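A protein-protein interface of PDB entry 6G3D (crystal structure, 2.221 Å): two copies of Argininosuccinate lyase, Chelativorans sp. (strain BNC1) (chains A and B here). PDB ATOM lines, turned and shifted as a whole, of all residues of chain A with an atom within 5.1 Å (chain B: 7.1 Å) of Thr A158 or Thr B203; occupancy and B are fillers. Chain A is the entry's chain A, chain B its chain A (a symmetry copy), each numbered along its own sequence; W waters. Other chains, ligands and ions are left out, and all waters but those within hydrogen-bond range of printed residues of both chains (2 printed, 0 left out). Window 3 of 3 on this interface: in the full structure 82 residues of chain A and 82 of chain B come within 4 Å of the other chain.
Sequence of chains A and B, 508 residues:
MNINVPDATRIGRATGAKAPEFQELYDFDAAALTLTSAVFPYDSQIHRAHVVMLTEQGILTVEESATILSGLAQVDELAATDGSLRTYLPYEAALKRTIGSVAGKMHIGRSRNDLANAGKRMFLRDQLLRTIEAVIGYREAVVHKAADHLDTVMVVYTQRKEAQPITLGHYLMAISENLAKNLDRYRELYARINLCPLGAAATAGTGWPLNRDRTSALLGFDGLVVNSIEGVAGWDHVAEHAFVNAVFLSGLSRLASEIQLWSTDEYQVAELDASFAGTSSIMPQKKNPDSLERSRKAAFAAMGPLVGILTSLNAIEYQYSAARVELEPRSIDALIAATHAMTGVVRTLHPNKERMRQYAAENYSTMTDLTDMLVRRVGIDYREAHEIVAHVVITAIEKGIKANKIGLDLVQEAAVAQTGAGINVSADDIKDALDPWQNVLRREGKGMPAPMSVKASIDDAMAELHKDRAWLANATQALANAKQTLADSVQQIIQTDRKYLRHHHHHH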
ATOM      1  N   VAL A 156      25.968   5.576  -0.148  1.00  0.00           N
ATOM      2  CA  VAL A 156      25.981   6.518   0.960  1.00  0.00           C
ATOM      3  C   VAL A 156      27.056   6.054   1.927  1.00  0.00           C
ATOM      4  O   VAL A 156      27.402   4.868   1.979  1.00  0.00           O
ATOM      5  CB  VAL A 156      24.600   6.601   1.642  1.00  0.00           C
ATOM      6  CG1 VAL A 156      24.250   5.262   2.265  1.00  0.00           C
ATOM      7  CG2 VAL A 156      24.557   7.734   2.669  1.00  0.00           C
ATOM      8  N   TYR A 157      27.603   6.988   2.692  1.00  0.00           N
ATOM      9  CA  TYR A 157      28.685   6.685   3.611  1.00  0.00           C
ATOM     10  C   TYR A 157      28.242   6.884   5.053  1.00  0.00           C
ATOM     11  O   TYR A 157      27.420   7.752   5.363  1.00  0.00           O
ATOM     12  CB  TYR A 157      29.910   7.562   3.337  1.00  0.00           C
ATOM     13  CG  TYR A 157      30.495   7.403   1.951  1.00  0.00           C
ATOM     14  CD1 TYR A 157      29.931   8.052   0.860  1.00  0.00           C
ATOM     15  CD2 TYR A 157      31.617   6.616   1.734  1.00  0.00           C
ATOM     16  CE1 TYR A 157      30.464   7.916  -0.410  1.00  0.00           C
ATOM     17  CE2 TYR A 157      32.157   6.474   0.467  1.00  0.00           C
ATOM     18  CZ  TYR A 157      31.578   7.127  -0.600  1.00  0.00           C
ATOM     19  OH  TYR A 157      32.117   6.984  -1.859  1.00  0.00           O
ATOM     20  N   THR A 158      28.789   6.048   5.928  1.00  0.00           N
ATOM     21  CA  THR A 158      28.789   6.289   7.360  1.00  0.00           C
ATOM     22  C   THR A 158      30.216   6.110   7.851  1.00  0.00           C
ATOM     23  O   THR A 158      30.902   5.160   7.458  1.00  0.00           O
ATOM     24  CB  THR A 158      27.852   5.345   8.127  1.00  0.00           C
ATOM     25  OG1 THR A 158      28.351   4.004   8.054  1.00  0.00           O
ATOM     26  CG2 THR A 158      26.439   5.398   7.564  1.00  0.00           C
ATOM     27  N   GLN A 159      30.660   7.044   8.691  1.00  0.00           N
ATOM     28  CA  GLN A 159      32.028   7.050   9.206  1.00  0.00           C
ATOM     29  C   GLN A 159      33.045   7.055   8.066  1.00  0.00           C
ATOM     30  O   GLN A 159      34.125   6.471   8.174  1.00  0.00           O
ATOM     31  CB  GLN A 159      32.264   5.867  10.152  1.00  0.00           C
ATOM     32  CG  GLN A 159      31.229   5.763  11.265  1.00  0.00           C
ATOM     33  CD  GLN A 159      31.599   4.749  12.330  1.00  0.00           C
ATOM     34  OE1 GLN A 159      31.058   3.645  12.371  1.00  0.00           O
ATOM     35  NE2 GLN A 159      32.520   5.128  13.208  1.00  0.00           N
ATOM     36  N   ARG A 160      32.684   7.715   6.962  1.00  0.00           N
ATOM     37  CA  ARG A 160      33.526   7.832   5.768  1.00  0.00           C
ATOM     38  C   ARG A 160      33.854   6.469   5.162  1.00  0.00           C
ATOM     39  O   ARG A 160      34.905   6.287   4.543  1.00  0.00           O
ATOM     40  CB  ARG A 160      34.806   8.619   6.067  1.00  0.00           C
ATOM     41  CG  ARG A 160      34.541  10.076   6.419  1.00  0.00           C
ATOM     42  CD  ARG A 160      35.813  10.809   6.819  1.00  0.00           C
ATOM     43  NE  ARG A 160      35.604  12.252   6.893  1.00  0.00           N
ATOM     44  CZ  ARG A 160      36.476  13.110   7.411  1.00  0.00           C
ATOM     45  NH1 ARG A 160      37.622  12.674   7.917  1.00  0.00           N
ATOM     46  NH2 ARG A 160      36.200  14.407   7.433  1.00  0.00           N
ATOM     47  N   LYS A 161      32.946   5.509   5.329  1.00  0.00           N
ATOM     48  CA  LYS A 161      33.049   4.189   4.723  1.00  0.00           C
ATOM     49  C   LYS A 161      31.772   3.892   3.952  1.00  0.00           C
ATOM     50  O   LYS A 161      30.678   4.262   4.390  1.00  0.00           O
ATOM     51  CB  LYS A 161      33.279   3.106   5.781  1.00  0.00           C
ATOM     52  CG  LYS A 161      34.720   2.974   6.234  1.00  0.00           C
ATOM     53  CD  LYS A 161      35.597   2.478   5.096  1.00  0.00           C
ATOM     54  CE  LYS A 161      36.876   1.845   5.618  1.00  0.00           C
ATOM     55  NZ  LYS A 161      37.657   1.221   4.510  1.00  0.00           N
ATOM     56  N   ALA A 163      28.522   2.411   2.821  1.00  0.00           N
ATOM     57  CA  ALA A 163      27.517   1.784   3.671  1.00  0.00           C
ATOM     58  C   ALA A 163      26.542   0.945   2.850  1.00  0.00           C
ATOM     59  O   ALA A 163      26.618  -0.285   2.874  1.00  0.00           O
ATOM     60  CB  ALA A 163      26.778   2.852   4.481  1.00  0.00           C
ATOM     61  N   HIS A 170      18.217  10.874  -3.446  1.00  0.00           N
ATOM     62  CA  HIS A 170      17.936  10.558  -2.048  1.00  0.00           C
ATOM     63  C   HIS A 170      18.833  11.362  -1.119  1.00  0.00           C
ATOM     64  O   HIS A 170      18.374  11.889  -0.098  1.00  0.00           O
ATOM     65  CB  HIS A 170      18.112   9.061  -1.788  1.00  0.00           C
ATOM     66  CG  HIS A 170      17.853   8.659  -0.366  1.00  0.00           C
ATOM     67  ND1 HIS A 170      18.828   8.112   0.440  1.00  0.00           N
ATOM     68  CD2 HIS A 170      16.729   8.716   0.390  1.00  0.00           C
ATOM     69  CE1 HIS A 170      18.318   7.849   1.630  1.00  0.00           C
ATOM     70  NE2 HIS A 170      17.046   8.206   1.626  1.00  0.00           N
ATOM     71  N   SER B 111      19.510  -0.645  13.026  1.00  0.00           N
ATOM     72  CA  SER B 111      20.938  -0.462  13.218  1.00  0.00           C
ATOM     73  C   SER B 111      21.165   0.117  14.605  1.00  0.00           C
ATOM     74  O   SER B 111      20.224   0.517  15.293  1.00  0.00           O
ATOM     75  CB  SER B 111      21.530   0.462  12.143  1.00  0.00           C
ATOM     76  OG  SER B 111      22.835   0.892  12.492  1.00  0.00           O
ATOM     77  N   ASN B 113      22.750   2.818  14.627  1.00  0.00           N
ATOM     78  CA  ASN B 113      22.782   4.230  14.261  1.00  0.00           C
ATOM     79  C   ASN B 113      21.434   4.901  14.504  1.00  0.00           C
ATOM     80  O   ASN B 113      21.369   5.974  15.113  1.00  0.00           O
ATOM     81  CB  ASN B 113      23.210   4.381  12.801  1.00  0.00           C
ATOM     82  CG  ASN B 113      24.599   3.821  12.542  1.00  0.00           C
ATOM     83  OD1 ASN B 113      25.383   3.632  13.472  1.00  0.00           O
ATOM     84  ND2 ASN B 113      24.913   3.566  11.277  1.00  0.00           N
ATOM     85  N   ASP B 114      20.341   4.294  14.033  1.00  0.00           N
ATOM     86  CA  ASP B 114      19.039   4.906  14.285  1.00  0.00           C
ATOM     87  C   ASP B 114      18.534   4.592  15.687  1.00  0.00           C
ATOM     88  O   ASP B 114      17.741   5.362  16.240  1.00  0.00           O
ATOM     89  CB  ASP B 114      18.014   4.474  13.229  1.00  0.00           C
ATOM     90  CG  ASP B 114      17.769   2.980  13.218  1.00  0.00           C
ATOM     91  OD1 ASP B 114      18.651   2.226  13.676  1.00  0.00           O
ATOM     92  OD2 ASP B 114      16.688   2.561  12.749  1.00  0.00           O
ATOM     93  N   GLY B 199      13.577   3.323  11.739  1.00  0.00           N
ATOM     94  CA  GLY B 199      13.269   2.958  10.377  1.00  0.00           C
ATOM     95  C   GLY B 199      14.303   3.415   9.373  1.00  0.00           C
ATOM     96  O   GLY B 199      14.318   2.905   8.246  1.00  0.00           O
ATOM     97  N   ALA B 200      15.158   4.369   9.747  1.00  0.00           N
ATOM     98  CA  ALA B 200      16.281   4.750   8.901  1.00  0.00           C
ATOM     99  C   ALA B 200      17.352   3.670   8.855  1.00  0.00           C
ATOM    100  O   ALA B 200      18.142   3.642   7.905  1.00  0.00           O
ATOM    101  CB  ALA B 200      16.897   6.063   9.391  1.00  0.00           C
ATOM    102  N   ALA B 201      17.389   2.792   9.855  1.00  0.00           N
ATOM    103  CA  ALA B 201      18.336   1.673   9.935  1.00  0.00           C
ATOM    104  C   ALA B 201      19.744   2.263   9.898  1.00  0.00           C
ATOM    105  O   ALA B 201      20.032   3.182  10.682  1.00  0.00           O
ATOM    106  CB  ALA B 201      18.020   0.650   8.850  1.00  0.00           C
ATOM    107  N   ALA B 202      20.635   1.786   9.026  1.00  0.00           N
ATOM    108  CA  ALA B 202      22.011   2.271   9.031  1.00  0.00           C
ATOM    109  C   ALA B 202      22.090   3.717   8.562  1.00  0.00           C
ATOM    110  O   ALA B 202      22.813   4.526   9.156  1.00  0.00           O
ATOM    111  CB  ALA B 202      22.887   1.374   8.157  1.00  0.00           C
ATOM    112  N   THR B 203      21.343   4.056   7.510  1.00  0.00           N
ATOM    113  CA  THR B 203      21.322   5.391   6.920  1.00  0.00           C
ATOM    114  C   THR B 203      20.419   5.418   5.696  1.00  0.00           C
ATOM    115  O   THR B 203      20.080   6.494   5.192  1.00  0.00           O
ATOM    116  CB  THR B 203      22.728   5.849   6.518  1.00  0.00           C
ATOM    117  OG1 THR B 203      22.650   7.113   5.852  1.00  0.00           O
ATOM    118  CG2 THR B 203      23.377   4.832   5.602  1.00  0.00           C
ATOM    119  N   ALA B 204      20.023   4.238   5.210  1.00  0.00           N
ATOM    120  CA  ALA B 204      19.331   4.127   3.931  1.00  0.00           C
ATOM    121  C   ALA B 204      18.066   3.280   4.019  1.00  0.00           C
ATOM    122  O   ALA B 204      17.600   2.769   2.996  1.00  0.00           O
ATOM    123  CB  ALA B 204      20.268   3.552   2.868  1.00  0.00           C
ATOM    124  N   GLY B 205      17.492   3.127   5.210  1.00  0.00           N
ATOM    125  CA  GLY B 205      16.277   2.346   5.321  1.00  0.00           C
ATOM    126  C   GLY B 205      16.559   0.855   5.245  1.00  0.00           C
ATOM    127  O   GLY B 205      17.647   0.379   5.585  1.00  0.00           O
ATOM    128  N   ASN B 227      13.500  11.478   5.958  1.00  0.00           N
ATOM    129  CA  ASN B 227      14.643  11.010   5.181  1.00  0.00           C
ATOM    130  C   ASN B 227      15.591  10.197   6.057  1.00  0.00           C
ATOM    131  O   ASN B 227      15.915  10.593   7.181  1.00  0.00           O
ATOM    132  CB  ASN B 227      15.374  12.197   4.551  1.00  0.00           C
ATOM    133  CG  ASN B 227      16.574  11.773   3.728  1.00  0.00           C
ATOM    134  OD1 ASN B 227      17.629  11.448   4.270  1.00  0.00           O
ATOM    135  ND2 ASN B 227      16.418  11.778   2.410  1.00  0.00           N
ATOM    136  N   SER B 228      16.038   9.054   5.529  1.00  0.00           N
ATOM    137  CA  SER B 228      16.786   8.098   6.339  1.00  0.00           C
ATOM    138  C   SER B 228      18.201   8.578   6.638  1.00  0.00           C
ATOM    139  O   SER B 228      18.748   8.252   7.697  1.00  0.00           O
ATOM    140  CB  SER B 228      16.815   6.736   5.643  1.00  0.00           C
ATOM    141  OG  SER B 228      17.457   6.822   4.383  1.00  0.00           O
ATOM    142  N   ILE B 229      18.814   9.332   5.725  1.00  0.00           N
ATOM    143  CA  ILE B 229      20.112   9.935   6.024  1.00  0.00           C
ATOM    144  C   ILE B 229      19.972  10.928   7.167  1.00  0.00           C
ATOM    145  O   ILE B 229      20.726  10.890   8.146  1.00  0.00           O
ATOM    146  CB  ILE B 229      20.709  10.602   4.772  1.00  0.00           C
ATOM    147  CG1 ILE B 229      21.040   9.560   3.704  1.00  0.00           C
ATOM    148  CG2 ILE B 229      21.954  11.399   5.140  1.00  0.00           C
ATOM    149  CD1 ILE B 229      21.074  10.116   2.301  1.00  0.00           C
ATOM    150  N   GLU B 230      18.988  11.827   7.060  1.00  0.00           N
ATOM    151  CA  GLU B 230      18.716  12.777   8.132  1.00  0.00           C
ATOM    152  C   GLU B 230      18.408  12.067   9.444  1.00  0.00           C
ATOM    153  O   GLU B 230      18.665  12.615  10.522  1.00  0.00           O
ATOM    154  CB  GLU B 230      17.551  13.687   7.731  1.00  0.00           C
ATOM    155  CG  GLU B 230      17.141  14.734   8.767  1.00  0.00           C
ATOM    156  CD  GLU B 230      18.168  15.842   8.957  1.00  0.00           C
ATOM    157  OE1 GLU B 230      19.289  15.745   8.412  1.00  0.00           O
ATOM    158  OE2 GLU B 230      17.853  16.826   9.658  1.00  0.00           O
ATOM    159  N   GLY B 231      17.874  10.847   9.372  1.00  0.00           N
ATOM    160  CA  GLY B 231      17.540  10.122  10.586  1.00  0.00           C
ATOM    161  C   GLY B 231      18.753   9.786  11.432  1.00  0.00           C
ATOM    162  O   GLY B 231      18.695   9.836  12.663  1.00  0.00           O
ATOM    163  N   VAL B 232      19.871   9.451  10.790  1.00  0.00           N
ATOM    164  CA  VAL B 232      21.060   9.021  11.518  1.00  0.00           C
ATOM    165  C   VAL B 232      22.096  10.138  11.555  1.00  0.00           C
ATOM    166  O   VAL B 232      22.915  10.206  12.480  1.00  0.00           O
ATOM    167  CB  VAL B 232      21.656   7.741  10.902  1.00  0.00           C
ATOM    168  CG1 VAL B 232      20.686   6.579  11.052  1.00  0.00           C
ATOM    169  CG2 VAL B 232      22.019   7.965   9.440  1.00  0.00           C
ATOM    170  N   ALA B 233      22.073  11.021  10.556  1.00  0.00           N
ATOM    171  CA  ALA B 233      23.050  12.098  10.474  1.00  0.00           C
ATOM    172  C   ALA B 233      22.581  13.388  11.128  1.00  0.00           C
ATOM    173  O   ALA B 233      23.419  14.222  11.491  1.00  0.00           O
ATOM    174  CB  ALA B 233      23.408  12.383   9.012  1.00  0.00           C
ATOM    175  N   TYR B 318      27.862  15.076   5.964  1.00  0.00           N
ATOM    176  CA  TYR B 318      26.476  14.878   6.385  1.00  0.00           C
ATOM    177  C   TYR B 318      26.173  13.380   6.418  1.00  0.00           C
ATOM    178  O   TYR B 318      25.398  12.835   5.631  1.00  0.00           O
ATOM    179  CB  TYR B 318      25.515  15.643   5.489  1.00  0.00           C
ATOM    180  CG  TYR B 318      24.333  16.134   6.280  1.00  0.00           C
ATOM    181  CD1 TYR B 318      24.414  17.301   7.026  1.00  0.00           C
ATOM    182  CD2 TYR B 318      23.159  15.401   6.334  1.00  0.00           C
ATOM    183  CE1 TYR B 318      23.347  17.742   7.771  1.00  0.00           C
ATOM    184  CE2 TYR B 318      22.086  15.835   7.078  1.00  0.00           C
ATOM    185  CZ  TYR B 318      22.186  17.005   7.794  1.00  0.00           C
ATOM    186  OH  TYR B 318      21.116  17.436   8.537  1.00  0.00           O
ATOM    187  N   GLN B 319      26.826  12.714   7.367  1.00  0.00           N
ATOM    188  CA  GLN B 319      26.738  11.274   7.526  1.00  0.00           C
ATOM    189  C   GLN B 319      26.490  10.960   8.989  1.00  0.00           C
ATOM    190  O   GLN B 319      26.625  11.825   9.859  1.00  0.00           O
ATOM    191  CB  GLN B 319      28.031  10.578   7.089  1.00  0.00           C
ATOM    192  CG  GLN B 319      28.507  10.909   5.697  1.00  0.00           C
ATOM    193  CD  GLN B 319      29.946  10.501   5.490  1.00  0.00           C
ATOM    194  OE1 GLN B 319      30.530   9.810   6.325  1.00  0.00           O
ATOM    195  NE2 GLN B 319      30.527  10.918   4.375  1.00  0.00           N
ATOM    196  N   TYR B 320      26.125   9.710   9.260  1.00  0.00           N
ATOM    197  CA  TYR B 320      26.299   9.210  10.612  1.00  0.00           C
ATOM    198  C   TYR B 320      27.781   9.236  10.939  1.00  0.00           C
ATOM    199  O   TYR B 320      28.622   8.908  10.102  1.00  0.00           O
ATOM    200  CB  TYR B 320      25.758   7.790  10.767  1.00  0.00           C
ATOM    201  CG  TYR B 320      26.224   7.165  12.061  1.00  0.00           C
ATOM    202  CD1 TYR B 320      25.561   7.423  13.251  1.00  0.00           C
ATOM    203  CD2 TYR B 320      27.351   6.347  12.103  1.00  0.00           C
ATOM    204  CE1 TYR B 320      25.993   6.874  14.440  1.00  0.00           C
ATOM    205  CE2 TYR B 320      27.791   5.796  13.287  1.00  0.00           C
ATOM    206  CZ  TYR B 320      27.107   6.060  14.453  1.00  0.00           C
ATOM    207  OH  TYR B 320      27.538   5.510  15.638  1.00  0.00           O
ATOM    208  N   SER B 321      28.106   9.633  12.162  1.00  0.00           N
ATOM    209  CA  SER B 321      29.499   9.748  12.559  1.00  0.00           C
ATOM    210  C   SER B 321      29.597   9.573  14.063  1.00  0.00           C
ATOM    211  O   SER B 321      28.798  10.154  14.801  1.00  0.00           O
ATOM    212  CB  SER B 321      30.077  11.103  12.138  1.00  0.00           C
ATOM    213  OG  SER B 321      31.350  11.316  12.722  1.00  0.00           O
HETATM  214  O   HOH W   1      28.004   2.314  10.438  1.00  0.00           O
HETATM  215  O   HOH W   2      25.084   8.666   6.493  1.00  0.00           O
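Of the 21 printed residues of chain B, 6 touch a printed residue of chain A.
Of the 8 printed residues of chain A, 6 touch a printed residue of chain B.
Printed residues of chain A that touch a printed residue of chain B: Val A156, Tyr A157, Thr A158, Gln A159, Arg A160 and His A170.
Hydrophobic or aromatic side chains of chain A within 4 Å of the printed part of chain B: Val A156, Tyr A157 and His A170.
Among the printed residues, no Asp or Glu carboxylate lies within 4 Å of a Lys or Arg side-chain nitrogen of the other chain.
No position is printed for both chains.
Water W2 lies within hydrogen-bond range of the backbone carbonyl oxygen of Tyr A157 (2.8 Å), the side-chain hydroxyl of Thr B203 (3.0 Å) and the backbone NH of Tyr B320 (3.1 Å).
Water W1 lies within hydrogen-bond range of the side-chain hydroxyl of Thr A158 and the side-chain amide nitrogen of Asn B113.
The backbone carbonyl oxygen of Val A156 lies within hydrogen-bond range of the backbone NH of Ala A163, at 2.8 Å.
The backbone carbonyl oxygen (O) of Thr B203 sits at hydrogen-bond distance from the side-chain hydroxyl (OG) of Ser B228.
The backbone NH (N) of Ile B229 lies within hydrogen-bond range of the backbone carbonyl oxygen (O) of Thr B203 (3.2 Å).
The side-chain amide oxygen (OD1) of Asn B227 sits at hydrogen-bond distance from the backbone NH (N) of Ile B229 (2.8 Å).
N of Glu B230 lies within hydrogen-bond range of OD1 of Asn B227.
Among the printed residues, merely in contact across the chains: Val A156 with Thr B203, Tyr A157 with Gln B319, Thr A158 with Thr B203, Thr A158 with Tyr B320, Gln A159 with Gln B319 and His A170 with Ile B229.
Printed residues of chain B within 4 Å of Tyr A157: Gln B319.
Printed residues of chain B within 4 Å of Thr A158: Thr B203 and Tyr B320.
Lys A161 touches none of the printed residues of chain B.
Thr B203 touches just these residues of chain A: Val A156 and Thr A158.
Val B232 touches none of the printed residues of chain A.
Printed residues of chain A within 4 Å of Gln B319: Tyr A157 (3.4 Å), Gln A159 (3.6 Å) and Arg A160 (3.1 Å).
Of the printed residues of chain A, Tyr B320 touches Thr A158 and Gln A159.
The nearest residue of chain A that does not touch Thr B203 is Ala A163 (4.1 Å).
The nearest printed residue of chain B that does not touch Val A156 is Ile B229 (4.1 Å).
NE2 of His A170 sits close to OG of Ser B228, 3.1 Å away.
N of Arg A160 is in hydrogen-bond range of OE1 of Gln B319, at 3.1 Å.
The backbone NH (N) of Gln A159 is in hydrogen-bond range of the backbone carbonyl oxygen (O) of Tyr B320 (3.1 Å).
The side-chain amide nitrogen (ND2) of Asn B227 lies within hydrogen-bond range of the backbone carbonyl oxygen (O) of His A170, at 3.2 Å.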
